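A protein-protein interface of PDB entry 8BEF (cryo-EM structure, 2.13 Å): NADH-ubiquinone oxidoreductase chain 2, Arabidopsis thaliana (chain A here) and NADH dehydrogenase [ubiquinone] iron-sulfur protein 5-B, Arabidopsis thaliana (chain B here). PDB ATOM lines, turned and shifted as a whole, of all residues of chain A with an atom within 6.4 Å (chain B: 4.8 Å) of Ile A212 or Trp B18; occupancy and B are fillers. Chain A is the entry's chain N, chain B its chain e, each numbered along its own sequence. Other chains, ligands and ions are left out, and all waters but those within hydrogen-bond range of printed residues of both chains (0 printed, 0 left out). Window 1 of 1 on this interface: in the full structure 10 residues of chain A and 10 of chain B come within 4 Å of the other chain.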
ATOM      1  N   SER A 200     -11.196  -7.441   0.597  1.00  0.00           N
ATOM      2  CA  SER A 200     -10.566  -7.611  -0.709  1.00  0.00           C
ATOM      3  C   SER A 200     -11.262  -6.806  -1.804  1.00  0.00           C
ATOM      4  O   SER A 200     -10.611  -6.365  -2.756  1.00  0.00           O
ATOM      5  CB  SER A 200     -10.532  -9.090  -1.081  1.00  0.00           C
ATOM      6  OG  SER A 200      -9.749  -9.832  -0.169  1.00  0.00           O
ATOM      7  N   THR A 201     -12.580  -6.614  -1.707  1.00  0.00           N
ATOM      8  CA  THR A 201     -13.322  -5.962  -2.779  1.00  0.00           C
ATOM      9  C   THR A 201     -13.897  -4.601  -2.416  1.00  0.00           C
ATOM     10  O   THR A 201     -14.292  -3.860  -3.320  1.00  0.00           O
ATOM     11  CB  THR A 201     -14.475  -6.857  -3.260  1.00  0.00           C
ATOM     12  OG1 THR A 201     -15.543  -6.825  -2.303  1.00  0.00           O
ATOM     13  CG2 THR A 201     -14.006  -8.283  -3.454  1.00  0.00           C
ATOM     14  N   GLY A 202     -13.899  -4.154  -1.197  1.00  0.00           N
ATOM     15  CA  GLY A 202     -14.628  -2.947  -0.846  1.00  0.00           C
ATOM     16  C   GLY A 202     -16.152  -3.025  -1.017  1.00  0.00           C
ATOM     17  O   GLY A 202     -16.773  -1.980  -0.964  1.00  0.00           O
ATOM     18  N   ALA A 203     -16.743  -4.214  -1.124  1.00  0.00           N
ATOM     19  CA  ALA A 203     -18.172  -4.305  -1.379  1.00  0.00           C
ATOM     20  C   ALA A 203     -18.789  -5.435  -0.564  1.00  0.00           C
ATOM     21  O   ALA A 203     -18.138  -6.438  -0.267  1.00  0.00           O
ATOM     22  CB  ALA A 203     -18.456  -4.526  -2.868  1.00  0.00           C
ATOM     23  N   ASP A 207     -24.824  -7.251  -6.061  1.00  0.00           N
ATOM     24  CA  ASP A 207     -24.593  -6.717  -7.404  1.00  0.00           C
ATOM     25  C   ASP A 207     -23.142  -6.286  -7.582  1.00  0.00           C
ATOM     26  O   ASP A 207     -22.499  -6.610  -8.591  1.00  0.00           O
ATOM     27  CB  ASP A 207     -25.522  -5.533  -7.664  1.00  0.00           C
ATOM     28  CG  ASP A 207     -26.833  -5.945  -8.278  1.00  0.00           C
ATOM     29  OD1 ASP A 207     -27.778  -5.132  -8.242  1.00  0.00           O
ATOM     30  OD2 ASP A 207     -26.926  -7.079  -8.787  1.00  0.00           O
ATOM     31  N   GLN A 208     -22.613  -5.545  -6.604  1.00  0.00           N
ATOM     32  CA  GLN A 208     -21.227  -5.100  -6.668  1.00  0.00           C
ATOM     33  C   GLN A 208     -20.274  -6.286  -6.701  1.00  0.00           C
ATOM     34  O   GLN A 208     -19.313  -6.299  -7.474  1.00  0.00           O
ATOM     35  CB  GLN A 208     -20.916  -4.194  -5.477  1.00  0.00           C
ATOM     36  CG  GLN A 208     -21.853  -3.005  -5.319  1.00  0.00           C
ATOM     37  CD  GLN A 208     -21.731  -2.334  -3.960  1.00  0.00           C
ATOM     38  OE1 GLN A 208     -21.316  -2.955  -2.983  1.00  0.00           O
ATOM     39  NE2 GLN A 208     -22.093  -1.059  -3.896  1.00  0.00           N
ATOM     40  N   LEU A 209     -20.534  -7.295  -5.866  1.00  0.00           N
ATOM     41  CA  LEU A 209     -19.704  -8.492  -5.861  1.00  0.00           C
ATOM     42  C   LEU A 209     -19.752  -9.198  -7.208  1.00  0.00           C
ATOM     43  O   LEU A 209     -18.725  -9.672  -7.706  1.00  0.00           O
ATOM     44  CB  LEU A 209     -20.152  -9.433  -4.745  1.00  0.00           C
ATOM     45  CG  LEU A 209     -19.918  -8.906  -3.326  1.00  0.00           C
ATOM     46  CD1 LEU A 209     -20.432  -9.891  -2.279  1.00  0.00           C
ATOM     47  CD2 LEU A 209     -18.447  -8.598  -3.117  1.00  0.00           C
ATOM     48  N   ALA A 210     -20.936  -9.270  -7.818  1.00  0.00           N
ATOM     49  CA  ALA A 210     -21.048  -9.875  -9.139  1.00  0.00           C
ATOM     50  C   ALA A 210     -20.198  -9.121 -10.155  1.00  0.00           C
ATOM     51  O   ALA A 210     -19.444  -9.729 -10.919  1.00  0.00           O
ATOM     52  CB  ALA A 210     -22.514  -9.919  -9.576  1.00  0.00           C
ATOM     53  N   LYS A 211     -20.282  -7.788 -10.156  1.00  0.00           N
ATOM     54  CA  LYS A 211     -19.510  -7.015 -11.127  1.00  0.00           C
ATOM     55  C   LYS A 211     -18.007  -7.194 -10.926  1.00  0.00           C
ATOM     56  O   LYS A 211     -17.266  -7.386 -11.897  1.00  0.00           O
ATOM     57  CB  LYS A 211     -19.886  -5.537 -11.052  1.00  0.00           C
ATOM     58  CG  LYS A 211     -21.136  -5.182 -11.831  1.00  0.00           C
ATOM     59  CD  LYS A 211     -21.647  -3.804 -11.455  1.00  0.00           C
ATOM     60  CE  LYS A 211     -22.677  -3.304 -12.451  1.00  0.00           C
ATOM     61  NZ  LYS A 211     -23.898  -4.149 -12.444  1.00  0.00           N
ATOM     62  N   ILE A 212     -17.538  -7.143  -9.677  1.00  0.00           N
ATOM     63  CA  ILE A 212     -16.102  -7.235  -9.417  1.00  0.00           C
ATOM     64  C   ILE A 212     -15.573  -8.608  -9.811  1.00  0.00           C
ATOM     65  O   ILE A 212     -14.529  -8.727 -10.462  1.00  0.00           O
ATOM     66  CB  ILE A 212     -15.791  -6.926  -7.941  1.00  0.00           C
ATOM     67  CG1 ILE A 212     -15.919  -5.435  -7.655  1.00  0.00           C
ATOM     68  CG2 ILE A 212     -14.383  -7.375  -7.590  1.00  0.00           C
ATOM     69  CD1 ILE A 212     -16.402  -5.127  -6.257  1.00  0.00           C
ATOM     70  N   LEU A 213     -16.231  -9.651  -9.336  1.00  0.00           N
ATOM     71  CA  LEU A 213     -15.737 -11.045  -9.526  1.00  0.00           C
ATOM     72  C   LEU A 213     -15.953 -11.618 -10.933  1.00  0.00           C
ATOM     73  O   LEU A 213     -15.226 -12.517 -11.240  1.00  0.00           O
ATOM     74  CB  LEU A 213     -16.372 -11.943  -8.460  1.00  0.00           C
ATOM     75  CG  LEU A 213     -16.194 -11.593  -6.985  1.00  0.00           C
ATOM     76  CD1 LEU A 213     -16.465 -12.815  -6.136  1.00  0.00           C
ATOM     77  CD2 LEU A 213     -14.807 -11.054  -6.688  1.00  0.00           C
ATOM     78  N   THR A 214     -16.826 -11.076 -11.771  1.00  0.00           N
ATOM     79  CA  THR A 214     -17.116 -11.699 -13.056  1.00  0.00           C
ATOM     80  C   THR A 214     -16.008 -11.425 -14.062  1.00  0.00           C
ATOM     81  O   THR A 214     -15.449 -10.326 -14.111  1.00  0.00           O
ATOM     82  CB  THR A 214     -18.448 -11.209 -13.625  1.00  0.00           C
ATOM     83  OG1 THR A 214     -18.607  -9.811 -13.363  1.00  0.00           O
ATOM     84  CG2 THR A 214     -19.606 -11.985 -13.012  1.00  0.00           C
ATOM     85  N   GLY A 215     -15.699 -12.437 -14.870  1.00  0.00           N
ATOM     86  CA  GLY A 215     -14.690 -12.335 -15.897  1.00  0.00           C
ATOM     87  C   GLY A 215     -13.286 -12.688 -15.467  1.00  0.00           C
ATOM     88  O   GLY A 215     -12.371 -12.638 -16.301  1.00  0.00           O
ATOM     89  N   TYR A 216     -13.072 -13.028 -14.206  1.00  0.00           N
ATOM     90  CA  TYR A 216     -11.704 -13.287 -13.770  1.00  0.00           C
ATOM     91  C   TYR A 216     -11.526 -14.618 -13.064  1.00  0.00           C
ATOM     92  O   TYR A 216     -10.529 -15.298 -13.320  1.00  0.00           O
ATOM     93  CB  TYR A 216     -11.224 -12.140 -12.869  1.00  0.00           C
ATOM     94  CG  TYR A 216     -11.108 -10.847 -13.623  1.00  0.00           C
ATOM     95  CD1 TYR A 216     -12.217 -10.039 -13.828  1.00  0.00           C
ATOM     96  CD2 TYR A 216      -9.894 -10.442 -14.155  1.00  0.00           C
ATOM     97  CE1 TYR A 216     -12.119  -8.870 -14.536  1.00  0.00           C
ATOM     98  CE2 TYR A 216      -9.785  -9.262 -14.859  1.00  0.00           C
ATOM     99  CZ  TYR A 216     -10.901  -8.480 -15.045  1.00  0.00           C
ATOM    100  OH  TYR A 216     -10.804  -7.301 -15.747  1.00  0.00           O
ATOM    101  N   ILE A 226     -10.336 -12.944  -1.548  1.00  0.00           N
ATOM    102  CA  ILE A 226     -11.618 -13.351  -2.180  1.00  0.00           C
ATOM    103  C   ILE A 226     -11.771 -14.876  -2.162  1.00  0.00           C
ATOM    104  O   ILE A 226     -12.834 -15.328  -1.733  1.00  0.00           O
ATOM    105  CB  ILE A 226     -11.739 -12.802  -3.604  1.00  0.00           C
ATOM    106  CG1 ILE A 226     -11.734 -11.274  -3.638  1.00  0.00           C
ATOM    107  CG2 ILE A 226     -12.978 -13.357  -4.296  1.00  0.00           C
ATOM    108  CD1 ILE A 226     -11.669 -10.710  -5.036  1.00  0.00           C
ATOM    109  N   ALA B   2     -16.998   0.628  -2.566  1.00  0.00           N
ATOM    110  CA  ALA B   2     -18.119   0.814  -3.503  1.00  0.00           C
ATOM    111  C   ALA B   2     -19.313   1.646  -3.034  1.00  0.00           C
ATOM    112  O   ALA B   2     -20.014   2.040  -3.857  1.00  0.00           O
ATOM    113  CB  ALA B   2     -18.524  -0.562  -3.974  1.00  0.00           C
ATOM    114  N   CYS B  14     -12.182   5.850  -3.156  1.00  0.00           N
ATOM    115  CA  CYS B  14     -12.234   4.983  -4.352  1.00  0.00           C
ATOM    116  C   CYS B  14     -13.614   4.904  -5.054  1.00  0.00           C
ATOM    117  O   CYS B  14     -13.729   4.174  -5.959  1.00  0.00           O
ATOM    118  CB  CYS B  14     -11.774   3.597  -3.930  1.00  0.00           C
ATOM    119  SG  CYS B  14     -10.130   3.604  -3.183  1.00  0.00           S
ATOM    120  N   TYR B  15     -14.557   5.708  -4.662  1.00  0.00           N
ATOM    121  CA  TYR B  15     -15.933   5.707  -5.200  1.00  0.00           C
ATOM    122  C   TYR B  15     -16.035   6.190  -6.669  1.00  0.00           C
ATOM    123  O   TYR B  15     -16.742   5.553  -7.363  1.00  0.00           O
ATOM    124  CB  TYR B  15     -16.842   6.510  -4.278  1.00  0.00           C
ATOM    125  CG  TYR B  15     -18.259   6.516  -4.760  1.00  0.00           C
ATOM    126  CD1 TYR B  15     -19.021   5.364  -4.692  1.00  0.00           C
ATOM    127  CD2 TYR B  15     -18.805   7.645  -5.336  1.00  0.00           C
ATOM    128  CE1 TYR B  15     -20.331   5.351  -5.126  1.00  0.00           C
ATOM    129  CE2 TYR B  15     -20.114   7.655  -5.774  1.00  0.00           C
ATOM    130  CZ  TYR B  15     -20.871   6.504  -5.659  1.00  0.00           C
ATOM    131  OH  TYR B  15     -22.138   6.490  -6.114  1.00  0.00           O
ATOM    132  N   ASP B  16     -15.277   7.184  -7.097  1.00  0.00           N
ATOM    133  CA  ASP B  16     -15.336   7.580  -8.499  1.00  0.00           C
ATOM    134  C   ASP B  16     -14.787   6.484  -9.406  1.00  0.00           C
ATOM    135  O   ASP B  16     -15.351   6.214 -10.473  1.00  0.00           O
ATOM    136  CB  ASP B  16     -14.594   8.898  -8.689  1.00  0.00           C
ATOM    137  CG  ASP B  16     -15.386  10.081  -8.163  1.00  0.00           C
ATOM    138  OD1 ASP B  16     -16.616   9.944  -8.014  1.00  0.00           O
ATOM    139  OD2 ASP B  16     -14.788  11.137  -7.882  1.00  0.00           O
ATOM    140  N   PHE B  17     -13.707   5.818  -8.986  1.00  0.00           N
ATOM    141  CA  PHE B  17     -13.203   4.672  -9.737  1.00  0.00           C
ATOM    142  C   PHE B  17     -14.246   3.566  -9.813  1.00  0.00           C
ATOM    143  O   PHE B  17     -14.460   2.969 -10.877  1.00  0.00           O
ATOM    144  CB  PHE B  17     -11.925   4.135  -9.091  1.00  0.00           C
ATOM    145  CG  PHE B  17     -10.713   4.982  -9.329  1.00  0.00           C
ATOM    146  CD1 PHE B  17     -10.149   5.079 -10.590  1.00  0.00           C
ATOM    147  CD2 PHE B  17     -10.117   5.665  -8.282  1.00  0.00           C
ATOM    148  CE1 PHE B  17      -9.025   5.858 -10.803  1.00  0.00           C
ATOM    149  CE2 PHE B  17      -8.994   6.443  -8.490  1.00  0.00           C
ATOM    150  CZ  PHE B  17      -8.449   6.540  -9.749  1.00  0.00           C
ATOM    151  N   TRP B  18     -14.871   3.280  -8.669  1.00  0.00           N
ATOM    152  CA  TRP B  18     -15.951   2.286  -8.642  1.00  0.00           C
ATOM    153  C   TRP B  18     -17.050   2.645  -9.663  1.00  0.00           C
ATOM    154  O   TRP B  18     -17.507   1.760 -10.301  1.00  0.00           O
ATOM    155  CB  TRP B  18     -16.539   2.102  -7.229  1.00  0.00           C
ATOM    156  CG  TRP B  18     -17.752   1.232  -7.291  1.00  0.00           C
ATOM    157  CD1 TRP B  18     -19.059   1.605  -7.188  1.00  0.00           C
ATOM    158  CD2 TRP B  18     -17.756  -0.164  -7.598  1.00  0.00           C
ATOM    159  NE1 TRP B  18     -19.871   0.524  -7.377  1.00  0.00           N
ATOM    160  CE2 TRP B  18     -19.103  -0.577  -7.624  1.00  0.00           C
ATOM    161  CE3 TRP B  18     -16.752  -1.103  -7.835  1.00  0.00           C
ATOM    162  CZ2 TRP B  18     -19.463  -1.893  -7.887  1.00  0.00           C
ATOM    163  CZ3 TRP B  18     -17.114  -2.398  -8.091  1.00  0.00           C
ATOM    164  CH2 TRP B  18     -18.451  -2.793  -8.109  1.00  0.00           C
ATOM    165  N   MET B  19     -17.478   3.876  -9.662  1.00  0.00           N
ATOM    166  CA  MET B  19     -18.598   4.268 -10.508  1.00  0.00           C
ATOM    167  C   MET B  19     -18.215   4.229 -11.981  1.00  0.00           C
ATOM    168  O   MET B  19     -19.032   3.842 -12.822  1.00  0.00           O
ATOM    169  CB  MET B  19     -19.103   5.652 -10.103  1.00  0.00           C
ATOM    170  CG  MET B  19     -19.792   5.668  -8.751  1.00  0.00           C
ATOM    171  SD  MET B  19     -21.071   4.406  -8.559  1.00  0.00           S
ATOM    172  CE  MET B  19     -22.382   5.119  -9.538  1.00  0.00           C
ATOM    173  N   ASP B  20     -16.978   4.609 -12.318  1.00  0.00           N
ATOM    174  CA  ASP B  20     -16.518   4.447 -13.697  1.00  0.00           C
ATOM    175  C   ASP B  20     -16.539   2.980 -14.108  1.00  0.00           C
ATOM    176  O   ASP B  20     -17.015   2.634 -15.196  1.00  0.00           O
ATOM    177  CB  ASP B  20     -15.112   5.026 -13.881  1.00  0.00           C
ATOM    178  CG  ASP B  20     -14.980   6.430 -13.351  1.00  0.00           C
ATOM    179  OD1 ASP B  20     -15.930   7.219 -13.519  1.00  0.00           O
ATOM    180  OD2 ASP B  20     -13.917   6.753 -12.777  1.00  0.00           O
ATOM    181  N   PHE B  21     -16.040   2.098 -13.239  1.00  0.00           N
ATOM    182  CA  PHE B  21     -16.034   0.674 -13.561  1.00  0.00           C
ATOM    183  C   PHE B  21     -17.452   0.130 -13.727  1.00  0.00           C
ATOM    184  O   PHE B  21     -17.730  -0.621 -14.671  1.00  0.00           O
ATOM    185  CB  PHE B  21     -15.284  -0.096 -12.476  1.00  0.00           C
ATOM    186  CG  PHE B  21     -15.442  -1.581 -12.565  1.00  0.00           C
ATOM    187  CD1 PHE B  21     -14.984  -2.274 -13.668  1.00  0.00           C
ATOM    188  CD2 PHE B  21     -16.044  -2.287 -11.534  1.00  0.00           C
ATOM    189  CE1 PHE B  21     -15.128  -3.643 -13.749  1.00  0.00           C
ATOM    190  CE2 PHE B  21     -16.187  -3.658 -11.610  1.00  0.00           C
ATOM    191  CZ  PHE B  21     -15.729  -4.336 -12.717  1.00  0.00           C
ATOM    192  N   SER B  22     -18.358   0.498 -12.817  1.00  0.00           N
ATOM    193  CA  SER B  22     -19.735   0.021 -12.891  1.00  0.00           C
ATOM    194  C   SER B  22     -20.432   0.533 -14.144  1.00  0.00           C
ATOM    195  O   SER B  22     -21.148  -0.219 -14.815  1.00  0.00           O
ATOM    196  CB  SER B  22     -20.510   0.445 -11.643  1.00  0.00           C
ATOM    197  OG  SER B  22     -19.906  -0.060 -10.468  1.00  0.00           O
ATOM    198  N   ARG B  38     -11.384  -1.604 -13.864  1.00  0.00           N
ATOM    199  CA  ARG B  38     -11.434  -2.495 -12.710  1.00  0.00           C
ATOM    200  C   ARG B  38     -10.110  -2.507 -11.956  1.00  0.00           C
ATOM    201  O   ARG B  38     -10.085  -2.450 -10.717  1.00  0.00           O
ATOM    202  CB  ARG B  38     -11.797  -3.905 -13.161  1.00  0.00           C
ATOM    203  CG  ARG B  38     -11.967  -4.895 -12.032  1.00  0.00           C
ATOM    204  CD  ARG B  38     -11.708  -6.292 -12.532  1.00  0.00           C
ATOM    205  NE  ARG B  38     -12.103  -7.325 -11.584  1.00  0.00           N
ATOM    206  CZ  ARG B  38     -11.248  -8.096 -10.926  1.00  0.00           C
ATOM    207  NH1 ARG B  38      -9.941  -7.974 -11.088  1.00  0.00           N
ATOM    208  NH2 ARG B  38     -11.717  -9.012 -10.085  1.00  0.00           N
ATOM    209  N   TYR B  41      -9.774   0.722  -9.965  1.00  0.00           N
ATOM    210  CA  TYR B  41     -10.541   0.585  -8.687  1.00  0.00           C
ATOM    211  C   TYR B  41      -9.743  -0.243  -7.659  1.00  0.00           C
ATOM    212  O   TYR B  41      -9.515   0.271  -6.610  1.00  0.00           O
ATOM    213  CB  TYR B  41     -11.948   0.044  -8.968  1.00  0.00           C
ATOM    214  CG  TYR B  41     -12.681  -0.327  -7.698  1.00  0.00           C
ATOM    215  CD1 TYR B  41     -13.110   0.650  -6.823  1.00  0.00           C
ATOM    216  CD2 TYR B  41     -12.874  -1.651  -7.338  1.00  0.00           C
ATOM    217  CE1 TYR B  41     -13.764   0.330  -5.646  1.00  0.00           C
ATOM    218  CE2 TYR B  41     -13.524  -1.998  -6.164  1.00  0.00           C
ATOM    219  CZ  TYR B  41     -13.970  -0.997  -5.314  1.00  0.00           C
ATOM    220  OH  TYR B  41     -14.611  -1.291  -4.155  1.00  0.00           O
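The backbone carbonyl oxygen (O) of Trp B18 sits close to the side-chain hydroxyl (OG) of Ser B22 (3.0 Å).
O of Lys A211 is in hydrogen-bond range of OG1 of Thr A214 (3.1 Å).
The backbone NH (N) of Ala B2 sits at hydrogen-bond distance from the side-chain hydroxyl (OH) of Tyr B41 (3.5 Å).
The side-chain hydroxyl of Thr A201 lies within hydrogen-bond range of the backbone NH of Ala A203.
O of Gly A202 sits at hydrogen-bond distance from N of Ala B2, 3.1 Å away.
The guanidinium group (NH2) of Arg B38 sits at hydrogen-bond distance from the backbone carbonyl oxygen (O) of Ile A212.
O of Thr A201 lies within hydrogen-bond range of OH of Tyr B41.
Gly A202 touches Tyr B41.
Gln A208 touches Ala B2 (NE2 to CB, 3.6 Å).
Trp B18 touches Gln A208.
Lys A211 touches Phe B21 (O to CZ, 3.5 Å).
CG1 of Ile A212 touches CZ3 of Trp B18, at 3.3 Å.
CE1 of Tyr A216 touches CD of Arg B38, 3.3 Å away.
Ile A212 touches just these residues of chain B: Trp B18 (3.3 Å) and Arg B38 (2.9 Å).
Of chain A, only Gln A208 (3.6 Å) and Ile A212 (3.3 Å) come within 4 Å of Trp B18.
Of the printed residues of chain B, Lys A211 touches Phe B21.
Printed residues of chain A within 4 Å of Ala B2: Gly A202 and Gln A208.
Of the printed residues of chain B, Tyr A216 touches Arg B38.
Leu A209 touches none of the printed residues of chain B.
Of the 12 printed residues of chain B, 5 touch a printed residue of chain A.
Hydrophobic or aromatic side chains of chain A within 4 Å of the printed part of chain B: Ile A212 and Tyr A216.
Along chain A the printed residues that touch a printed residue of chain B span positions 201 to 216.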
